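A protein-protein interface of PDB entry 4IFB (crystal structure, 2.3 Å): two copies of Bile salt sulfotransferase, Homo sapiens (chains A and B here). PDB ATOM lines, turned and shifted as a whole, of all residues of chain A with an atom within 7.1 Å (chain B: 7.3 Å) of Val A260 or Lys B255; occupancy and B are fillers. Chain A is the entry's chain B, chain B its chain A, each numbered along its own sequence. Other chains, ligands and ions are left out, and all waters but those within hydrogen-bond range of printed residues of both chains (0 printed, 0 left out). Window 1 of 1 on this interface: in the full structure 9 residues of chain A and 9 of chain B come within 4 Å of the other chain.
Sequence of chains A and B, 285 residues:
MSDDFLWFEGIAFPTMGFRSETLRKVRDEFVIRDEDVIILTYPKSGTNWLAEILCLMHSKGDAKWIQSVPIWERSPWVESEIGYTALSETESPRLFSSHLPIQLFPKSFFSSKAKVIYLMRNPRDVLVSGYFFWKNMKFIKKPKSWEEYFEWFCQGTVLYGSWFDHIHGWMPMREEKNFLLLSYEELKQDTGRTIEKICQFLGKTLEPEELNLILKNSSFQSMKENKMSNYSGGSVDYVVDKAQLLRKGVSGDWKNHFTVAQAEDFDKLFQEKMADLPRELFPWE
Thr B259 touches His A257 (CG2 to N, 3.9 Å). O of Phe A258 touches CA of Thr B259, 3.1 Å away. O of Lys B255 touches CB of Thr A259, 3.5 Å away. Thr A259 touches Asn B256 (CG2 to O, 3.5 Å). Thr A259 touches Phe B258. Trp B254 touches Val A260. Val A260 touches Thr B259. Val A260 touches Ala B263 (CG2 to CB, 3.5 Å). Ala A261 touches Asn B256. Ala A263 touches Val B260.
O of Lys B255 sits at hydrogen-bond distance from N of Ala A261. N of Val B260 sits at hydrogen-bond distance from O of Phe A258, 3.1 Å away. The backbone carbonyl oxygen (O) of Phe B258 sits at hydrogen-bond distance from the backbone NH (N) of Val A260. N of Val A260 lies within hydrogen-bond range of O of Lys B255.
The backbone NH (N) of Thr B259 sits at hydrogen-bond distance from the side-chain amide oxygen (OE1) of Gln B262. The side-chain amide oxygen (OE1) of Gln A262 lies within hydrogen-bond range of the backbone NH (N) of Thr A259 (2.9 Å). N of Trp B254 is in hydrogen-bond range of OD1 of Asp B125 (2.9 Å). OG1 of Thr B259 sits close to N of Ala B261. OG1 of Thr A259 lies close to N of Ala A261, at 3.4 Å. The side-chain carboxylate (OE2) of Glu B285 sits at hydrogen-bond distance from the indole nitrogen (NE1) of Trp B254, at 3.4 Å.
Of the 17 printed residues of chain B, 7 touch a printed residue of chain A. Hydrophobic or aromatic side chains of chain B within 4 Å of the printed part of chain A: Trp B254, Val B260 and Ala B263. Printed residues of chain A that touch a printed residue of chain B: His A257, Phe A258, Thr A259, Val A260, Ala A261 and Ala A263. Hydrophobic or aromatic side chains of chain A within 4 Å of the printed part of chain B: Val A260, Ala A261 and Ala A263. Among the printed residues, no Asp or Glu carboxylate lies within 4 Å of a Lys or Arg side-chain nitrogen of the other chain.
Of the printed residues of chain B, Val A260 touches Trp B254 (3.99 Å), Lys B255 (3.3 Å), Phe B258 (2.9 Å), Thr B259 (3.9 Å) and Ala B263 (3.5 Å). Lys B255 touches just these residues of chain A: Thr A259, Val A260 and Ala A261. Printed residues of chain A within 4 Å of Ala B263: Val A260. Of the printed residues of chain B, His A257 touches Thr B259 (3.9 Å). Printed residues of chain A within 4 Å of Asn B256: Thr A259 (3.5 Å) and Ala A261 (3.6 Å). Of the printed residues of chain A, Phe B258 touches Thr A259 (3.1 Å) and Val A260 (2.9 Å). Val B128 touches none of the printed residues of chain A. The nearest printed residue of chain B that does not touch Val A260 is Val B260 (4.5 Å). The nearest residue of chain A that does not touch Lys B255 is Glu A264 (4.2 Å).
Phe A258 touches Thr B259, and with the chains exchanged Thr A259 touches Phe B258. Phe A258 touches Val B260, and with the chains exchanged Val A260 touches Phe B258. Val A260 touches Thr B259, but with the chains exchanged Thr A259 does not touch Val B260 (4.1 Å). Val A260 touches Ala B263, and with the chains exchanged Ala A263 touches Val B260. Positions printed for both chains: 257, 258, 259, 260, 261, 262, 263 and 264. Of the 14 pairs that touch across the chains among the printed residues, 6 have their exchanged pair printed and touching as well.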
ATOM      1  N   HIS A 257      11.740  13.406  25.895  1.00  0.00           N
ATOM      2  CA  HIS A 257      11.078  14.135  24.810  1.00  0.00           C
ATOM      3  C   HIS A 257      10.050  13.295  24.067  1.00  0.00           C
ATOM      4  O   HIS A 257       9.006  13.786  23.726  1.00  0.00           O
ATOM      5  CB  HIS A 257      12.085  14.772  23.854  1.00  0.00           C
ATOM      6  CG  HIS A 257      13.029  15.718  24.525  1.00  0.00           C
ATOM      7  ND1 HIS A 257      12.760  17.062  24.666  1.00  0.00           N
ATOM      8  CD2 HIS A 257      14.242  15.517  25.091  1.00  0.00           C
ATOM      9  CE1 HIS A 257      13.762  17.650  25.296  1.00  0.00           C
ATOM     10  NE2 HIS A 257      14.680  16.737  25.558  1.00  0.00           N
ATOM     11  N   PHE A 258      10.329  12.028  23.835  1.00  0.00           N
ATOM     12  CA  PHE A 258       9.305  11.170  23.266  1.00  0.00           C
ATOM     13  C   PHE A 258       8.121  11.089  24.233  1.00  0.00           C
ATOM     14  O   PHE A 258       8.316  10.779  25.415  1.00  0.00           O
ATOM     15  CB  PHE A 258       9.854   9.762  22.978  1.00  0.00           C
ATOM     16  CG  PHE A 258      10.604   9.669  21.682  1.00  0.00           C
ATOM     17  CD1 PHE A 258      11.471  10.703  21.281  1.00  0.00           C
ATOM     18  CD2 PHE A 258      10.406   8.600  20.815  1.00  0.00           C
ATOM     19  CE1 PHE A 258      12.189  10.597  20.106  1.00  0.00           C
ATOM     20  CE2 PHE A 258      11.089   8.525  19.600  1.00  0.00           C
ATOM     21  CZ  PHE A 258      11.972   9.525  19.249  1.00  0.00           C
ATOM     22  N   THR A 259       6.907  11.371  23.758  1.00  0.00           N
ATOM     23  CA  THR A 259       5.750  11.060  24.600  1.00  0.00           C
ATOM     24  C   THR A 259       5.670   9.546  24.590  1.00  0.00           C
ATOM     25  O   THR A 259       6.397   8.908  23.817  1.00  0.00           O
ATOM     26  CB  THR A 259       4.428  11.656  24.073  1.00  0.00           C
ATOM     27  OG1 THR A 259       4.102  11.039  22.832  1.00  0.00           O
ATOM     28  CG2 THR A 259       4.541  13.164  23.885  1.00  0.00           C
ATOM     29  N   VAL A 260       4.825   8.976  25.453  1.00  0.00           N
ATOM     30  CA  VAL A 260       4.600   7.519  25.501  1.00  0.00           C
ATOM     31  C   VAL A 260       4.036   6.982  24.171  1.00  0.00           C
ATOM     32  O   VAL A 260       4.311   5.843  23.782  1.00  0.00           O
ATOM     33  CB  VAL A 260       3.700   7.064  26.712  1.00  0.00           C
ATOM     34  CG1 VAL A 260       3.419   5.556  26.673  1.00  0.00           C
ATOM     35  CG2 VAL A 260       4.345   7.401  28.064  1.00  0.00           C
ATOM     36  N   ALA A 261       3.225   7.789  23.496  1.00  0.00           N
ATOM     37  CA  ALA A 261       2.590   7.334  22.258  1.00  0.00           C
ATOM     38  C   ALA A 261       3.626   7.378  21.137  1.00  0.00           C
ATOM     39  O   ALA A 261       3.773   6.401  20.411  1.00  0.00           O
ATOM     40  CB  ALA A 261       1.356   8.181  21.904  1.00  0.00           C
ATOM     41  N   GLN A 262       4.373   8.476  21.031  1.00  0.00           N
ATOM     42  CA  GLN A 262       5.530   8.488  20.141  1.00  0.00           C
ATOM     43  C   GLN A 262       6.467   7.288  20.370  1.00  0.00           C
ATOM     44  O   GLN A 262       6.760   6.533  19.441  1.00  0.00           O
ATOM     45  CB  GLN A 262       6.272   9.819  20.211  1.00  0.00           C
ATOM     46  CG  GLN A 262       5.411  10.988  19.798  1.00  0.00           C
ATOM     47  CD  GLN A 262       6.008  12.327  20.184  1.00  0.00           C
ATOM     48  OE1 GLN A 262       6.806  12.432  21.112  1.00  0.00           O
ATOM     49  NE2 GLN A 262       5.653  13.363  19.439  1.00  0.00           N
ATOM     50  N   ALA A 263       6.888   7.047  21.600  1.00  0.00           N
ATOM     51  CA  ALA A 263       7.684   5.836  21.837  1.00  0.00           C
ATOM     52  C   ALA A 263       7.028   4.576  21.270  1.00  0.00           C
ATOM     53  O   ALA A 263       7.722   3.697  20.744  1.00  0.00           O
ATOM     54  CB  ALA A 263       7.987   5.647  23.316  1.00  0.00           C
ATOM     55  N   GLU A 264       5.714   4.424  21.441  1.00  0.00           N
ATOM     56  CA  GLU A 264       5.044   3.221  20.918  1.00  0.00           C
ATOM     57  C   GLU A 264       5.088   3.194  19.378  1.00  0.00           C
ATOM     58  O   GLU A 264       5.385   2.168  18.794  1.00  0.00           O
ATOM     59  CB  GLU A 264       3.588   3.157  21.360  1.00  0.00           C
ATOM     60  CG  GLU A 264       3.288   2.111  22.418  1.00  0.00           C
ATOM     61  CD  GLU A 264       2.259   2.599  23.438  1.00  0.00           C
ATOM     62  OE1 GLU A 264       1.188   3.116  23.021  1.00  0.00           O
ATOM     63  OE2 GLU A 264       2.532   2.483  24.658  1.00  0.00           O
ATOM     64  N   ASP A 265       4.768   4.311  18.730  1.00  0.00           N
ATOM     65  CA  ASP A 265       4.852   4.382  17.277  1.00  0.00           C
ATOM     66  C   ASP A 265       6.258   4.061  16.770  1.00  0.00           C
ATOM     67  O   ASP A 265       6.417   3.220  15.901  1.00  0.00           O
ATOM     68  CB  ASP A 265       4.410   5.744  16.760  1.00  0.00           C
ATOM     69  CG  ASP A 265       2.956   6.012  17.035  1.00  0.00           C
ATOM     70  OD1 ASP A 265       2.211   5.023  17.256  1.00  0.00           O
ATOM     71  OD2 ASP A 265       2.574   7.213  17.051  1.00  0.00           O
ATOM     72  N   ARG B 124      -3.061  10.442  35.911  1.00  0.00           N
ATOM     73  CA  ARG B 124      -2.294  10.879  34.735  1.00  0.00           C
ATOM     74  C   ARG B 124      -3.185  11.686  33.803  1.00  0.00           C
ATOM     75  O   ARG B 124      -2.799  12.757  33.349  1.00  0.00           O
ATOM     76  CB  ARG B 124      -1.637   9.703  34.008  1.00  0.00           C
ATOM     77  CG  ARG B 124      -0.856   8.757  34.930  1.00  0.00           C
ATOM     78  CD  ARG B 124      -0.584   7.443  34.210  1.00  0.00           C
ATOM     79  NE  ARG B 124       0.190   6.480  34.984  1.00  0.00           N
ATOM     80  CZ  ARG B 124      -0.290   5.760  35.989  1.00  0.00           C
ATOM     81  NH1 ARG B 124      -1.552   5.939  36.421  1.00  0.00           N
ATOM     82  NH2 ARG B 124       0.513   4.893  36.604  1.00  0.00           N
ATOM     83  N   ASP B 125      -4.428  11.258  33.639  1.00  0.00           N
ATOM     84  CA  ASP B 125      -5.393  12.010  32.828  1.00  0.00           C
ATOM     85  C   ASP B 125      -5.835  13.307  33.534  1.00  0.00           C
ATOM     86  O   ASP B 125      -5.999  14.361  32.895  1.00  0.00           O
ATOM     87  CB  ASP B 125      -6.588  11.116  32.465  1.00  0.00           C
ATOM     88  CG  ASP B 125      -6.233  10.047  31.421  1.00  0.00           C
ATOM     89  OD1 ASP B 125      -5.260  10.261  30.674  1.00  0.00           O
ATOM     90  OD2 ASP B 125      -6.914   8.983  31.340  1.00  0.00           O
ATOM     91  N   VAL B 128      -3.056  15.964  33.000  1.00  0.00           N
ATOM     92  CA  VAL B 128      -3.154  16.559  31.667  1.00  0.00           C
ATOM     93  C   VAL B 128      -4.276  17.586  31.574  1.00  0.00           C
ATOM     94  O   VAL B 128      -4.080  18.736  31.107  1.00  0.00           O
ATOM     95  CB  VAL B 128      -3.351  15.464  30.594  1.00  0.00           C
ATOM     96  CG1 VAL B 128      -3.578  16.094  29.223  1.00  0.00           C
ATOM     97  CG2 VAL B 128      -2.115  14.565  30.557  1.00  0.00           C
ATOM     98  N   GLY B 252      -6.995   7.971  28.676  1.00  0.00           N
ATOM     99  CA  GLY B 252      -5.767   7.544  27.986  1.00  0.00           C
ATOM    100  C   GLY B 252      -5.016   8.666  27.279  1.00  0.00           C
ATOM    101  O   GLY B 252      -3.909   8.466  26.770  1.00  0.00           O
ATOM    102  N   ASP B 253      -5.567   9.871  27.287  1.00  0.00           N
ATOM    103  CA  ASP B 253      -4.842  10.999  26.711  1.00  0.00           C
ATOM    104  C   ASP B 253      -3.459  11.269  27.372  1.00  0.00           C
ATOM    105  O   ASP B 253      -2.637  11.997  26.829  1.00  0.00           O
ATOM    106  CB  ASP B 253      -5.678  12.275  26.768  1.00  0.00           C
ATOM    107  CG  ASP B 253      -5.138  13.334  25.838  1.00  0.00           C
ATOM    108  OD1 ASP B 253      -5.042  14.529  26.239  1.00  0.00           O
ATOM    109  OD2 ASP B 253      -4.785  12.933  24.689  1.00  0.00           O
ATOM    110  N   TRP B 254      -3.249  10.785  28.594  1.00  0.00           N
ATOM    111  CA  TRP B 254      -1.980  11.055  29.250  1.00  0.00           C
ATOM    112  C   TRP B 254      -0.803  10.559  28.375  1.00  0.00           C
ATOM    113  O   TRP B 254       0.232  11.209  28.297  1.00  0.00           O
ATOM    114  CB  TRP B 254      -1.944  10.447  30.650  1.00  0.00           C
ATOM    115  CG  TRP B 254      -1.954   8.964  30.665  1.00  0.00           C
ATOM    116  CD1 TRP B 254      -3.057   8.151  30.649  1.00  0.00           C
ATOM    117  CD2 TRP B 254      -0.812   8.096  30.680  1.00  0.00           C
ATOM    118  NE1 TRP B 254      -2.666   6.814  30.665  1.00  0.00           N
ATOM    119  CE2 TRP B 254      -1.296   6.763  30.696  1.00  0.00           C
ATOM    120  CE3 TRP B 254       0.576   8.320  30.728  1.00  0.00           C
ATOM    121  CZ2 TRP B 254      -0.448   5.660  30.731  1.00  0.00           C
ATOM    122  CZ3 TRP B 254       1.418   7.236  30.767  1.00  0.00           C
ATOM    123  CH2 TRP B 254       0.905   5.907  30.761  1.00  0.00           C
ATOM    124  N   LYS B 255      -1.011   9.456  27.659  1.00  0.00           N
ATOM    125  CA  LYS B 255      -0.024   8.953  26.690  1.00  0.00           C
ATOM    126  C   LYS B 255       0.495   9.941  25.644  1.00  0.00           C
ATOM    127  O   LYS B 255       1.650   9.830  25.211  1.00  0.00           O
ATOM    128  CB  LYS B 255      -0.503   7.671  26.025  1.00  0.00           C
ATOM    129  CG  LYS B 255      -0.606   6.558  27.042  1.00  0.00           C
ATOM    130  CD  LYS B 255      -0.992   5.233  26.418  1.00  0.00           C
ATOM    131  CE  LYS B 255      -1.251   4.207  27.513  1.00  0.00           C
ATOM    132  NZ  LYS B 255      -0.896   2.825  27.083  1.00  0.00           N
ATOM    133  N   ASN B 256      -0.316  10.909  25.256  1.00  0.00           N
ATOM    134  CA  ASN B 256       0.104  11.863  24.254  1.00  0.00           C
ATOM    135  C   ASN B 256       0.868  12.989  24.884  1.00  0.00           C
ATOM    136  O   ASN B 256       1.183  13.985  24.219  1.00  0.00           O
ATOM    137  CB  ASN B 256      -1.113  12.422  23.500  1.00  0.00           C
ATOM    138  CG  ASN B 256      -1.929  11.320  22.846  1.00  0.00           C
ATOM    139  OD1 ASN B 256      -1.382  10.455  22.155  1.00  0.00           O
ATOM    140  ND2 ASN B 256      -3.211  11.266  23.168  1.00  0.00           N
ATOM    141  N   HIS B 257       1.084  12.907  26.192  1.00  0.00           N
ATOM    142  CA  HIS B 257       1.695  14.042  26.869  1.00  0.00           C
ATOM    143  C   HIS B 257       2.836  13.674  27.815  1.00  0.00           C
ATOM    144  O   HIS B 257       3.758  14.450  27.991  1.00  0.00           O
ATOM    145  CB  HIS B 257       0.637  14.894  27.566  1.00  0.00           C
ATOM    146  CG  HIS B 257      -0.342  15.515  26.620  1.00  0.00           C
ATOM    147  ND1 HIS B 257      -0.094  16.703  25.967  1.00  0.00           N
ATOM    148  CD2 HIS B 257      -1.545  15.081  26.171  1.00  0.00           C
ATOM    149  CE1 HIS B 257      -1.094  16.972  25.142  1.00  0.00           C
ATOM    150  NE2 HIS B 257      -1.995  16.013  25.260  1.00  0.00           N
ATOM    151  N   PHE B 258       2.749  12.533  28.474  1.00  0.00           N
ATOM    152  CA  PHE B 258       3.837  12.143  29.354  1.00  0.00           C
ATOM    153  C   PHE B 258       4.985  11.733  28.457  1.00  0.00           C
ATOM    154  O   PHE B 258       4.773  10.965  27.508  1.00  0.00           O
ATOM    155  CB  PHE B 258       3.443  10.940  30.236  1.00  0.00           C
ATOM    156  CG  PHE B 258       2.689  11.314  31.504  1.00  0.00           C
ATOM    157  CD1 PHE B 258       1.681  12.283  31.485  1.00  0.00           C
ATOM    158  CD2 PHE B 258       2.917  10.619  32.695  1.00  0.00           C
ATOM    159  CE1 PHE B 258       0.937  12.570  32.614  1.00  0.00           C
ATOM    160  CE2 PHE B 258       2.185  10.920  33.838  1.00  0.00           C
ATOM    161  CZ  PHE B 258       1.213  11.913  33.804  1.00  0.00           C
ATOM    162  N   THR B 259       6.196  12.187  28.789  1.00  0.00           N
ATOM    163  CA  THR B 259       7.417  11.593  28.229  1.00  0.00           C
ATOM    164  C   THR B 259       7.611  10.223  28.802  1.00  0.00           C
ATOM    165  O   THR B 259       6.931   9.846  29.759  1.00  0.00           O
ATOM    166  CB  THR B 259       8.665  12.406  28.538  1.00  0.00           C
ATOM    167  OG1 THR B 259       8.885  12.376  29.952  1.00  0.00           O
ATOM    168  CG2 THR B 259       8.510  13.851  28.046  1.00  0.00           C
ATOM    169  N   VAL B 260       8.503   9.438  28.201  1.00  0.00           N
ATOM    170  CA  VAL B 260       8.704   8.074  28.684  1.00  0.00           C
ATOM    171  C   VAL B 260       9.242   8.163  30.117  1.00  0.00           C
ATOM    172  O   VAL B 260       8.885   7.335  30.972  1.00  0.00           O
ATOM    173  CB  VAL B 260       9.698   7.298  27.786  1.00  0.00           C
ATOM    174  CG1 VAL B 260       9.957   5.913  28.328  1.00  0.00           C
ATOM    175  CG2 VAL B 260       9.197   7.222  26.349  1.00  0.00           C
ATOM    176  N   ALA B 261      10.110   9.155  30.375  1.00  0.00           N
ATOM    177  CA  ALA B 261      10.763   9.267  31.687  1.00  0.00           C
ATOM    178  C   ALA B 261       9.720   9.639  32.763  1.00  0.00           C
ATOM    179  O   ALA B 261       9.655   8.980  33.803  1.00  0.00           O
ATOM    180  CB  ALA B 261      11.909  10.288  31.663  1.00  0.00           C
ATOM    181  N   GLN B 262       8.900  10.666  32.479  1.00  0.00           N
ATOM    182  CA  GLN B 262       7.730  11.004  33.304  1.00  0.00           C
ATOM    183  C   GLN B 262       6.786   9.819  33.543  1.00  0.00           C
ATOM    184  O   GLN B 262       6.433   9.547  34.675  1.00  0.00           O
ATOM    185  CB  GLN B 262       6.966  12.153  32.695  1.00  0.00           C
ATOM    186  CG  GLN B 262       7.760  13.446  32.626  1.00  0.00           C
ATOM    187  CD  GLN B 262       7.048  14.489  31.785  1.00  0.00           C
ATOM    188  OE1 GLN B 262       6.127  14.181  31.021  1.00  0.00           O
ATOM    189  NE2 GLN B 262       7.487  15.722  31.892  1.00  0.00           N
ATOM    190  N   ALA B 263       6.443   9.066  32.502  1.00  0.00           N
ATOM    191  CA  ALA B 263       5.701   7.822  32.704  1.00  0.00           C
ATOM    192  C   ALA B 263       6.374   6.918  33.700  1.00  0.00           C
ATOM    193  O   ALA B 263       5.716   6.369  34.604  1.00  0.00           O
ATOM    194  CB  ALA B 263       5.482   7.075  31.400  1.00  0.00           C
ATOM    195  N   GLU B 264       7.673   6.704  33.514  1.00  0.00           N
ATOM    196  CA  GLU B 264       8.419   5.814  34.404  1.00  0.00           C
ATOM    197  C   GLU B 264       8.456   6.331  35.856  1.00  0.00           C
ATOM    198  O   GLU B 264       8.231   5.561  36.795  1.00  0.00           O
ATOM    199  CB  GLU B 264       9.846   5.602  33.898  1.00  0.00           C
ATOM    200  CG  GLU B 264      10.129   4.208  33.343  1.00  0.00           C
ATOM    201  CD  GLU B 264      11.101   4.230  32.155  1.00  0.00           C
ATOM    202  OE1 GLU B 264      12.146   4.939  32.213  1.00  0.00           O
ATOM    203  OE2 GLU B 264      10.811   3.538  31.149  1.00  0.00           O
ATOM    204  N   GLU B 285      -4.661   0.870  33.837  1.00  0.00           N
ATOM    205  CA  GLU B 285      -3.266   0.463  33.776  1.00  0.00           C
ATOM    206  C   GLU B 285      -2.396   1.334  34.694  1.00  0.00           C
ATOM    207  O   GLU B 285      -1.540   0.831  35.427  1.00  0.00           O
ATOM    208  CB  GLU B 285      -2.788   0.543  32.299  1.00  0.00           C
ATOM    209  CG  GLU B 285      -2.755   1.948  31.631  1.00  0.00           C
ATOM    210  CD  GLU B 285      -4.115   2.557  31.192  1.00  0.00           C
ATOM    211  OE1 GLU B 285      -5.169   1.865  31.165  1.00  0.00           O
ATOM    212  OE2 GLU B 285      -4.131   3.765  30.858  1.00  0.00           O
